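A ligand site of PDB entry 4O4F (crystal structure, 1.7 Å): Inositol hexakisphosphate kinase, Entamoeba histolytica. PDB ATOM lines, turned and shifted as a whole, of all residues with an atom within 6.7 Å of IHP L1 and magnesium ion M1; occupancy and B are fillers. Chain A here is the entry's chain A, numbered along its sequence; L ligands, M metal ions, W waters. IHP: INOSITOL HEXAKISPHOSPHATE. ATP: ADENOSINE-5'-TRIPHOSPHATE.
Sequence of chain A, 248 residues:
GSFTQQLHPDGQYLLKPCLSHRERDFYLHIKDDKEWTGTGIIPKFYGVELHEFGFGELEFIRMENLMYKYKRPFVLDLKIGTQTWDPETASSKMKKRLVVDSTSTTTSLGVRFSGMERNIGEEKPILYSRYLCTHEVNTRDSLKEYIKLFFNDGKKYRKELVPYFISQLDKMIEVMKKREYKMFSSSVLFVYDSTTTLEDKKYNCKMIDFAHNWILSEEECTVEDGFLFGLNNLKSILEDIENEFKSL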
ATOM      1  N   GLY A   1     -17.939   7.991  -7.454  1.00  0.00           N
ATOM      2  CA  GLY A   1     -19.035   7.718  -8.426  1.00  0.00           C
ATOM      3  C   GLY A   1     -20.408   8.243  -8.032  1.00  0.00           C
ATOM      4  O   GLY A   1     -21.346   8.129  -8.809  1.00  0.00           O
ATOM      5  N   SER A   2     -20.534   8.810  -6.828  1.00  0.00           N
ATOM      6  CA  SER A   2     -21.828   9.306  -6.342  1.00  0.00           C
ATOM      7  C   SER A   2     -22.135  10.730  -6.843  1.00  0.00           C
ATOM      8  O   SER A   2     -23.251  11.215  -6.679  1.00  0.00           O
ATOM      9  CB  SER A   2     -21.919   9.202  -4.813  1.00  0.00           C
ATOM     10  OG  SER A   2     -21.010  10.068  -4.157  1.00  0.00           O
ATOM     11  N   GLN A   5     -17.299  13.868 -10.907  1.00  0.00           N
ATOM     12  CA  GLN A   5     -16.045  14.024 -10.149  1.00  0.00           C
ATOM     13  C   GLN A   5     -15.215  15.270 -10.479  1.00  0.00           C
ATOM     14  O   GLN A   5     -14.213  15.537  -9.811  1.00  0.00           O
ATOM     15  CB  GLN A   5     -15.184  12.748 -10.248  1.00  0.00           C
ATOM     16  CG  GLN A   5     -15.838  11.541  -9.582  1.00  0.00           C
ATOM     17  CD  GLN A   5     -14.844  10.469  -9.181  1.00  0.00           C
ATOM     18  OE1 GLN A   5     -13.773  10.319  -9.777  1.00  0.00           O
ATOM     19  NE2 GLN A   5     -15.192   9.692  -8.144  1.00  0.00           N
ATOM     20  N   LYS A  16     -21.663  16.091  -0.754  1.00  0.00           N
ATOM     21  CA  LYS A  16     -21.591  14.665  -1.053  1.00  0.00           C
ATOM     22  C   LYS A  16     -22.735  13.893  -0.449  1.00  0.00           C
ATOM     23  O   LYS A  16     -22.948  13.943   0.737  1.00  0.00           O
ATOM     24  CB  LYS A  16     -20.253  14.116  -0.559  1.00  0.00           C
ATOM     25  CG  LYS A  16     -20.004  12.679  -0.928  1.00  0.00           C
ATOM     26  CD  LYS A  16     -18.666  12.186  -0.390  1.00  0.00           C
ATOM     27  CE  LYS A  16     -18.507  10.702  -0.709  1.00  0.00           C
ATOM     28  NZ  LYS A  16     -17.229  10.157  -0.194  1.00  0.00           N
ATOM     29  N   ASP A  77      -4.469  11.011  -6.339  1.00  0.00           N
ATOM     30  CA  ASP A  77      -5.188  10.266  -5.323  1.00  0.00           C
ATOM     31  C   ASP A  77      -4.404   8.995  -5.029  1.00  0.00           C
ATOM     32  O   ASP A  77      -4.133   8.208  -5.948  1.00  0.00           O
ATOM     33  CB  ASP A  77      -6.584   9.909  -5.815  1.00  0.00           C
ATOM     34  CG  ASP A  77      -7.418   9.246  -4.761  1.00  0.00           C
ATOM     35  OD1 ASP A  77      -7.076   8.116  -4.376  1.00  0.00           O
ATOM     36  OD2 ASP A  77      -8.433   9.833  -4.290  1.00  0.00           O
ATOM     37  N   LYS A  79      -4.562   5.613  -2.642  1.00  0.00           N
ATOM     38  CA  LYS A  79      -5.442   4.819  -1.802  1.00  0.00           C
ATOM     39  C   LYS A  79      -4.578   4.153  -0.721  1.00  0.00           C
ATOM     40  O   LYS A  79      -3.503   3.603  -1.034  1.00  0.00           O
ATOM     41  CB  LYS A  79      -6.170   3.783  -2.660  1.00  0.00           C
ATOM     42  CG  LYS A  79      -7.480   3.306  -2.091  1.00  0.00           C
ATOM     43  CD  LYS A  79      -8.229   2.404  -3.040  1.00  0.00           C
ATOM     44  CE  LYS A  79      -9.021   3.183  -4.083  1.00  0.00           C
ATOM     45  NZ  LYS A  79      -9.568   2.250  -5.107  1.00  0.00           N
ATOM     46  N   SER A  92     -19.368 -10.495  -4.748  1.00  0.00           N
ATOM     47  CA  SER A  92     -19.192 -10.389  -6.196  1.00  0.00           C
ATOM     48  C   SER A  92     -18.017  -9.491  -6.567  1.00  0.00           C
ATOM     49  O   SER A  92     -17.498  -9.599  -7.692  1.00  0.00           O
ATOM     50  CB  SER A  92     -20.458  -9.865  -6.845  1.00  0.00           C
ATOM     51  OG  SER A  92     -20.678  -8.529  -6.519  1.00  0.00           O
ATOM     52  N   LYS A  93     -17.583  -8.635  -5.635  1.00  0.00           N
ATOM     53  CA  LYS A  93     -16.404  -7.763  -5.831  1.00  0.00           C
ATOM     54  C   LYS A  93     -15.054  -8.318  -5.355  1.00  0.00           C
ATOM     55  O   LYS A  93     -14.018  -7.738  -5.663  1.00  0.00           O
ATOM     56  CB  LYS A  93     -16.627  -6.431  -5.129  1.00  0.00           C
ATOM     57  CG  LYS A  93     -17.925  -5.710  -5.513  1.00  0.00           C
ATOM     58  CD  LYS A  93     -17.953  -5.404  -6.993  1.00  0.00           C
ATOM     59  CE  LYS A  93     -19.270  -4.775  -7.428  1.00  0.00           C
ATOM     60  NZ  LYS A  93     -19.349  -4.675  -8.904  1.00  0.00           N
ATOM     61  N   LYS A  96     -11.920  -9.533  -7.597  1.00  0.00           N
ATOM     62  CA  LYS A  96     -11.218  -8.372  -8.147  1.00  0.00           C
ATOM     63  C   LYS A  96     -10.464  -7.609  -7.065  1.00  0.00           C
ATOM     64  O   LYS A  96      -9.351  -7.155  -7.298  1.00  0.00           O
ATOM     65  CB  LYS A  96     -12.215  -7.428  -8.774  1.00  0.00           C
ATOM     66  CG  LYS A  96     -11.566  -6.204  -9.355  1.00  0.00           C
ATOM     67  CD  LYS A  96     -12.444  -5.531 -10.382  1.00  0.00           C
ATOM     68  CE  LYS A  96     -13.279  -4.429  -9.792  1.00  0.00           C
ATOM     69  NZ  LYS A  96     -13.148  -3.221 -10.656  1.00  0.00           N
ATOM     70  N   ARG A  97     -11.078  -7.416  -5.889  1.00  0.00           N
ATOM     71  CA  ARG A  97     -10.431  -6.642  -4.829  1.00  0.00           C
ATOM     72  C   ARG A  97      -9.118  -7.315  -4.434  1.00  0.00           C
ATOM     73  O   ARG A  97      -8.104  -6.651  -4.251  1.00  0.00           O
ATOM     74  CB  ARG A  97     -11.301  -6.503  -3.565  1.00  0.00           C
ATOM     75  CG  ARG A  97     -12.525  -5.608  -3.719  1.00  0.00           C
ATOM     76  CD  ARG A  97     -12.215  -4.113  -3.729  1.00  0.00           C
ATOM     77  NE  ARG A  97     -13.512  -3.420  -3.732  1.00  0.00           N
ATOM     78  CZ  ARG A  97     -14.276  -3.217  -4.806  1.00  0.00           C
ATOM     79  NH1 ARG A  97     -13.844  -3.532  -6.034  1.00  0.00           N
ATOM     80  NH2 ARG A  97     -15.465  -2.638  -4.667  1.00  0.00           N
ATOM     81  N   VAL A 100      -6.470  -6.931  -7.339  1.00  0.00           N
ATOM     82  CA  VAL A 100      -5.965  -5.564  -7.470  1.00  0.00           C
ATOM     83  C   VAL A 100      -5.066  -5.234  -6.285  1.00  0.00           C
ATOM     84  O   VAL A 100      -3.976  -4.661  -6.475  1.00  0.00           O
ATOM     85  CB  VAL A 100      -7.070  -4.504  -7.692  1.00  0.00           C
ATOM     86  CG1 VAL A 100      -6.478  -3.094  -7.725  1.00  0.00           C
ATOM     87  CG2 VAL A 100      -7.817  -4.761  -8.988  1.00  0.00           C
ATOM     88  N   ARG A 112      -1.254   2.761  -2.760  1.00  0.00           N
ATOM     89  CA  ARG A 112      -1.208   2.573  -4.213  1.00  0.00           C
ATOM     90  C   ARG A 112      -1.687   3.797  -4.988  1.00  0.00           C
ATOM     91  O   ARG A 112      -2.538   4.597  -4.520  1.00  0.00           O
ATOM     92  CB  ARG A 112      -1.971   1.311  -4.624  1.00  0.00           C
ATOM     93  CG  ARG A 112      -3.501   1.399  -4.575  1.00  0.00           C
ATOM     94  CD  ARG A 112      -4.057   0.343  -5.525  1.00  0.00           C
ATOM     95  NE  ARG A 112      -5.517   0.205  -5.549  1.00  0.00           N
ATOM     96  CZ  ARG A 112      -6.210  -0.763  -4.959  1.00  0.00           C
ATOM     97  NH1 ARG A 112      -5.627  -1.662  -4.205  1.00  0.00           N
ATOM     98  NH2 ARG A 112      -7.543  -0.806  -5.090  1.00  0.00           N
ATOM     99  N   SER A 114      -3.763   5.832  -7.423  1.00  0.00           N
ATOM    100  CA  SER A 114      -5.170   5.800  -7.730  1.00  0.00           C
ATOM    101  C   SER A 114      -5.711   6.927  -8.581  1.00  0.00           C
ATOM    102  O   SER A 114      -6.799   7.326  -8.411  1.00  0.00           O
ATOM    103  CB  SER A 114      -6.005   5.600  -6.472  1.00  0.00           C
ATOM    104  OG  SER A 114      -7.202   4.944  -6.742  1.00  0.00           O
ATOM    105  N   ARG A 130      -6.472   5.557 -12.841  1.00  0.00           N
ATOM    106  CA  ARG A 130      -6.285   4.775 -11.603  1.00  0.00           C
ATOM    107  C   ARG A 130      -5.848   3.341 -11.886  1.00  0.00           C
ATOM    108  O   ARG A 130      -5.140   2.706 -11.094  1.00  0.00           O
ATOM    109  CB  ARG A 130      -7.562   4.792 -10.775  1.00  0.00           C
ATOM    110  CG  ARG A 130      -8.759   4.109 -11.424  1.00  0.00           C
ATOM    111  CD  ARG A 130     -10.007   4.255 -10.578  1.00  0.00           C
ATOM    112  NE  ARG A 130     -11.153   3.585 -11.194  1.00  0.00           N
ATOM    113  CZ  ARG A 130     -12.246   4.186 -11.669  1.00  0.00           C
ATOM    114  NH1 ARG A 130     -12.409   5.500 -11.569  1.00  0.00           N
ATOM    115  NH2 ARG A 130     -13.221   3.459 -12.224  1.00  0.00           N
ATOM    116  N   TYR A 131      -6.245   2.817 -13.043  1.00  0.00           N
ATOM    117  CA  TYR A 131      -5.879   1.441 -13.405  1.00  0.00           C
ATOM    118  C   TYR A 131      -4.396   1.189 -13.707  1.00  0.00           C
ATOM    119  O   TYR A 131      -3.960   0.032 -13.818  1.00  0.00           O
ATOM    120  CB  TYR A 131      -6.792   0.945 -14.554  1.00  0.00           C
ATOM    121  CG  TYR A 131      -8.236   0.916 -14.125  1.00  0.00           C
ATOM    122  CD1 TYR A 131      -8.645   0.066 -13.116  1.00  0.00           C
ATOM    123  CD2 TYR A 131      -9.181   1.778 -14.667  1.00  0.00           C
ATOM    124  CE1 TYR A 131      -9.954   0.047 -12.675  1.00  0.00           C
ATOM    125  CE2 TYR A 131     -10.504   1.775 -14.239  1.00  0.00           C
ATOM    126  CZ  TYR A 131     -10.888   0.892 -13.248  1.00  0.00           C
ATOM    127  OH  TYR A 131     -12.199   0.854 -12.775  1.00  0.00           O
ATOM    128  N   SER A 185     -10.261   1.653   1.760  1.00  0.00           N
ATOM    129  CA  SER A 185     -10.484   2.329   0.477  1.00  0.00           C
ATOM    130  C   SER A 185     -10.542   3.850   0.603  1.00  0.00           C
ATOM    131  O   SER A 185     -11.071   4.527  -0.296  1.00  0.00           O
ATOM    132  CB  SER A 185     -11.745   1.788  -0.240  1.00  0.00           C
ATOM    133  OG  SER A 185     -11.588   0.450  -0.693  1.00  0.00           O
ATOM    134  N   ASP A 209     -12.652  10.279   1.787  1.00  0.00           N
ATOM    135  CA  ASP A 209     -13.433   9.112   1.401  1.00  0.00           C
ATOM    136  C   ASP A 209     -13.584   8.096   2.511  1.00  0.00           C
ATOM    137  O   ASP A 209     -12.867   7.091   2.577  1.00  0.00           O
ATOM    138  CB  ASP A 209     -12.965   8.467   0.121  1.00  0.00           C
ATOM    139  CG  ASP A 209     -13.983   7.467  -0.389  1.00  0.00           C
ATOM    140  OD1 ASP A 209     -15.104   7.303   0.226  1.00  0.00           O
ATOM    141  OD2 ASP A 209     -13.654   6.826  -1.381  1.00  0.00           O
HETATM  142  C1  IHP L   1     -15.567   0.354  -9.111  1.00  0.00           C
HETATM  143  C2  IHP L   1     -16.629   1.260  -9.483  1.00  0.00           C
HETATM  144  C3  IHP L   1     -16.821   2.614  -8.975  1.00  0.00           C
HETATM  145  C4  IHP L   1     -15.526   3.366  -8.842  1.00  0.00           C
HETATM  146  C5  IHP L   1     -14.284   2.516  -8.712  1.00  0.00           C
HETATM  147  C6  IHP L   1     -14.252   1.059  -9.099  1.00  0.00           C
HETATM  148  O11 IHP L   1     -15.647  -1.089  -9.233  1.00  0.00           O
HETATM  149  P1  IHP L   1     -16.402  -2.204  -8.386  1.00  0.00           P
HETATM  150  O21 IHP L   1     -15.370  -3.308  -8.362  1.00  0.00           O
HETATM  151  O31 IHP L   1     -17.555  -2.538  -9.306  1.00  0.00           O
HETATM  152  O41 IHP L   1     -16.733  -1.559  -7.063  1.00  0.00           O
HETATM  153  O12 IHP L   1     -16.817   1.085 -10.836  1.00  0.00           O
HETATM  154  P2  IHP L   1     -18.006   0.382 -11.629  1.00  0.00           P
HETATM  155  O22 IHP L   1     -17.780   0.946 -13.013  1.00  0.00           O
HETATM  156  O32 IHP L   1     -17.677  -1.088 -11.499  1.00  0.00           O
HETATM  157  O42 IHP L   1     -19.272   0.864 -10.956  1.00  0.00           O
HETATM  158  O13 IHP L   1     -17.989   3.396  -8.950  1.00  0.00           O
HETATM  159  P3  IHP L   1     -19.326   3.136  -8.104  1.00  0.00           P
HETATM  160  O23 IHP L   1     -18.863   2.974  -6.664  1.00  0.00           O
HETATM  161  O33 IHP L   1     -19.902   1.887  -8.712  1.00  0.00           O
HETATM  162  O43 IHP L   1     -20.112   4.409  -8.362  1.00  0.00           O
HETATM  163  O14 IHP L   1     -15.588   4.436  -7.904  1.00  0.00           O
HETATM  164  P4  IHP L   1     -15.382   5.916  -8.522  1.00  0.00           P
HETATM  165  O24 IHP L   1     -16.489   6.034  -9.548  1.00  0.00           O
HETATM  166  O34 IHP L   1     -13.978   5.987  -9.093  1.00  0.00           O
HETATM  167  O44 IHP L   1     -15.529   6.805  -7.297  1.00  0.00           O
HETATM  168  O15 IHP L   1     -13.013   3.082  -8.587  1.00  0.00           O
HETATM  169  P5  IHP L   1     -12.160   3.661  -7.348  1.00  0.00           P
HETATM  170  O25 IHP L   1     -12.899   3.445  -6.040  1.00  0.00           O
HETATM  171  O35 IHP L   1     -11.905   5.099  -7.703  1.00  0.00           O
HETATM  172  O45 IHP L   1     -10.898   2.835  -7.497  1.00  0.00           O
HETATM  173  O16 IHP L   1     -13.251   0.310  -8.419  1.00  0.00           O
HETATM  174  P6  IHP L   1     -11.966  -0.047  -9.297  1.00  0.00           P
HETATM  175  O26 IHP L   1     -11.164  -0.977  -8.422  1.00  0.00           O
HETATM  176  O36 IHP L   1     -11.273   1.292  -9.530  1.00  0.00           O
HETATM  177  O46 IHP L   1     -12.489  -0.666 -10.599  1.00  0.00           O
HETATM  178  PG  ATP L   2     -17.509   6.840  -2.335  1.00  0.00           P
HETATM  179  O1G ATP L   2     -17.262   7.540  -1.015  1.00  0.00           O
HETATM  180  O2G ATP L   2     -16.241   6.452  -3.072  1.00  0.00           O
HETATM  181  O3G ATP L   2     -18.557   5.757  -2.286  1.00  0.00           O
HETATM  182  PB  ATP L   2     -17.390   9.013  -4.292  1.00  0.00           P
HETATM  183  O1B ATP L   2     -16.426   8.287  -5.214  1.00  0.00           O
HETATM  184  O2B ATP L   2     -18.535   9.781  -4.894  1.00  0.00           O
HETATM  185  O3B ATP L   2     -18.153   8.006  -3.263  1.00  0.00           O
HETATM  186  PA  ATP L   2     -15.037  10.349  -3.080  1.00  0.00           P
HETATM  187  O1A ATP L   2     -14.996  10.964  -1.691  1.00  0.00           O
HETATM  188  O2A ATP L   2     -14.253   9.105  -3.418  1.00  0.00           O
HETATM  189  O3A ATP L   2     -16.605  10.124  -3.394  1.00  0.00           O
HETATM  190  O5' ATP L   2     -14.592  11.509  -4.090  1.00  0.00           O
HETATM  191  C5' ATP L   2     -14.350  11.265  -5.482  1.00  0.00           C
HETATM  192  C4' ATP L   2     -13.240  12.172  -6.013  1.00  0.00           C
HETATM  193  O4' ATP L   2     -13.556  13.553  -5.823  1.00  0.00           O
HETATM  194  C3' ATP L   2     -11.895  11.953  -5.329  1.00  0.00           C
HETATM  195  O3' ATP L   2     -11.135  10.923  -5.972  1.00  0.00           O
HETATM  196  C2' ATP L   2     -11.223  13.305  -5.458  1.00  0.00           C
HETATM  197  O2' ATP L   2     -10.545  13.429  -6.716  1.00  0.00           O
HETATM  198  C1' ATP L   2     -12.369  14.294  -5.443  1.00  0.00           C
HETATM  199  N9  ATP L   2     -12.642  14.831  -4.088  1.00  0.00           N
HETATM  200  C8  ATP L   2     -13.167  14.169  -3.056  1.00  0.00           C
HETATM  201  N7  ATP L   2     -13.325  14.960  -1.990  1.00  0.00           N
HETATM  202  C5  ATP L   2     -12.930  16.188  -2.372  1.00  0.00           C
HETATM  203  C6  ATP L   2     -12.863  17.527  -1.772  1.00  0.00           C
HETATM  204  N6  ATP L   2     -13.257  17.731  -0.503  1.00  0.00           N
HETATM  205  N1  ATP L   2     -12.378  18.530  -2.512  1.00  0.00           N
HETATM  206  C2  ATP L   2     -11.958  18.358  -3.801  1.00  0.00           C
HETATM  207  N3  ATP L   2     -12.000  17.149  -4.414  1.00  0.00           N
HETATM  208  C4  ATP L   2     -12.478  16.086  -3.746  1.00  0.00           C
HETATM  209 MG    MG M   1     -15.899   6.275  -5.232  1.00  0.00          MG
HETATM  210 MG    MG M   2     -14.299   5.310  -2.839  1.00  0.00          MG
HETATM  211  O   HOH W   1     -14.086   7.062  -4.620  1.00  0.00           O
HETATM  212  O   HOH W   2     -13.198   0.789  -4.731  1.00  0.00           O
HETATM  213  O   HOH W   3     -12.139   4.470  -3.303  1.00  0.00           O
HETATM  214  O   HOH W   4     -11.650   6.953  -5.874  1.00  0.00           O
HETATM  215  O   HOH W   5      -8.826   0.138  -7.728  1.00  0.00           O
HETATM  216  O   HOH W   6     -17.694   5.416  -5.865  1.00  0.00           O
HETATM  217  O   HOH W   7     -10.956  -3.497  -6.918  1.00  0.00           O
HETATM  218  O   HOH W   8      -9.439   6.152  -7.506  1.00  0.00           O
HETATM  219  O   HOH W   9     -15.257   4.420  -5.043  1.00  0.00           O
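Hydrophobic or aromatic side chains within 4 Å of IHP L1: Tyr 131. Along chain A the residues within 4 Å of IHP L1 span positions 1 to 131. The nearest printed residue that does not touch IHP L1 is Ser 114 (4.3 Å).
Water W6 bridges O23 of IHP L1 (2.8 Å) and N of Gly 1 (3.0 Å). Water W5 lies within hydrogen-bond range of an oxygen (O26) of IHP L1, the guanidinium group of Arg 112 and the side-chain amino group of Lys 79. Water W8 bridges OG of Ser 114 and O35 of IHP L1. Water W7 bridges an oxygen (O26) of IHP L1 (2.9 Å) and the guanidinium group (NH1) of Arg 97 (3.0 Å). Water W3 lies within hydrogen-bond range of an oxygen (O25) of IHP L1 (3.0 Å) and the backbone carbonyl oxygen of Ser 185 (3.2 Å).
Residues that only touch magnesium ion M1: Gly 1 (3.5 Å). Of the 17 residues printed, 1 comes within 4 Å of magnesium ion M1. The nearest printed residue that does not touch magnesium ion M1 is Asp 209 (4.5 Å).
Magnesium ion M1 is bound by water W9 (2.0 Å), water W1 (2.1 Å), O1B of ATP L2 (2.1 Å), water W6 (2.1 Å), O44 of IHP L1 (2.2 Å) and O2G of ATP L2 (2.2 Å). Magnesium ion M1 has six donor atoms within binding distance.
The side-chain hydroxyl of Tyr 131 is in hydrogen-bond range of the guanidinium group of Arg 130 (2.9 Å). NE2 of Gln 5 sits close to N of Gly 1 (3.3 Å). O of Arg 112 lies within hydrogen-bond range of N of Lys 79, at 2.9 Å.
The side-chain amino group (NZ) of Lys 96 lies within salt-bridge range of an oxygen (O46) of IHP L1 (2.6 Å). O46 of IHP L1 sits at hydrogen-bond distance from OH of Tyr 131, at 2.7 Å. N of Gly 1 lies within hydrogen-bond range of O24 of IHP L1. O21 of IHP L1 lies within salt-bridge range of NH1 of Arg 97 (2.8 Å). The side-chain amino group (NZ) of Lys 79 lies within salt-bridge range of an oxygen (O45) of IHP L1, at 2.8 Å. O31 of IHP L1 lies within salt-bridge range of NZ of Lys 93 (2.8 Å). The guanidinium group of Arg 130 lies within salt-bridge range of an oxygen (O36) of IHP L1 (2.8 Å). O44 of IHP L1 lies close to NE2 of Gln 5 (3.0 Å). An oxygen (O2B) of ATP L2 lies within hydrogen-bond range of the backbone NH (N) of Gly 1. O1B of ATP L2 lies close to NE2 of Gln 5 (3.5 Å). The backbone NH (N) of Ser 2 is in hydrogen-bond range of an oxygen (O2B) of ATP L2 (2.9 Å). The side-chain hydroxyl (OG) of Ser 2 sits at hydrogen-bond distance from an oxygen (O2B) of ATP L2 (2.6 Å). The side-chain amino group (NZ) of Lys 16 is in salt-bridge range of an oxygen (O1G) of ATP L2 (2.7 Å). The side-chain carboxylate of Asp 77 lies within hydrogen-bond range of an oxygen (O3') of ATP L2, at 3.4 Å.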
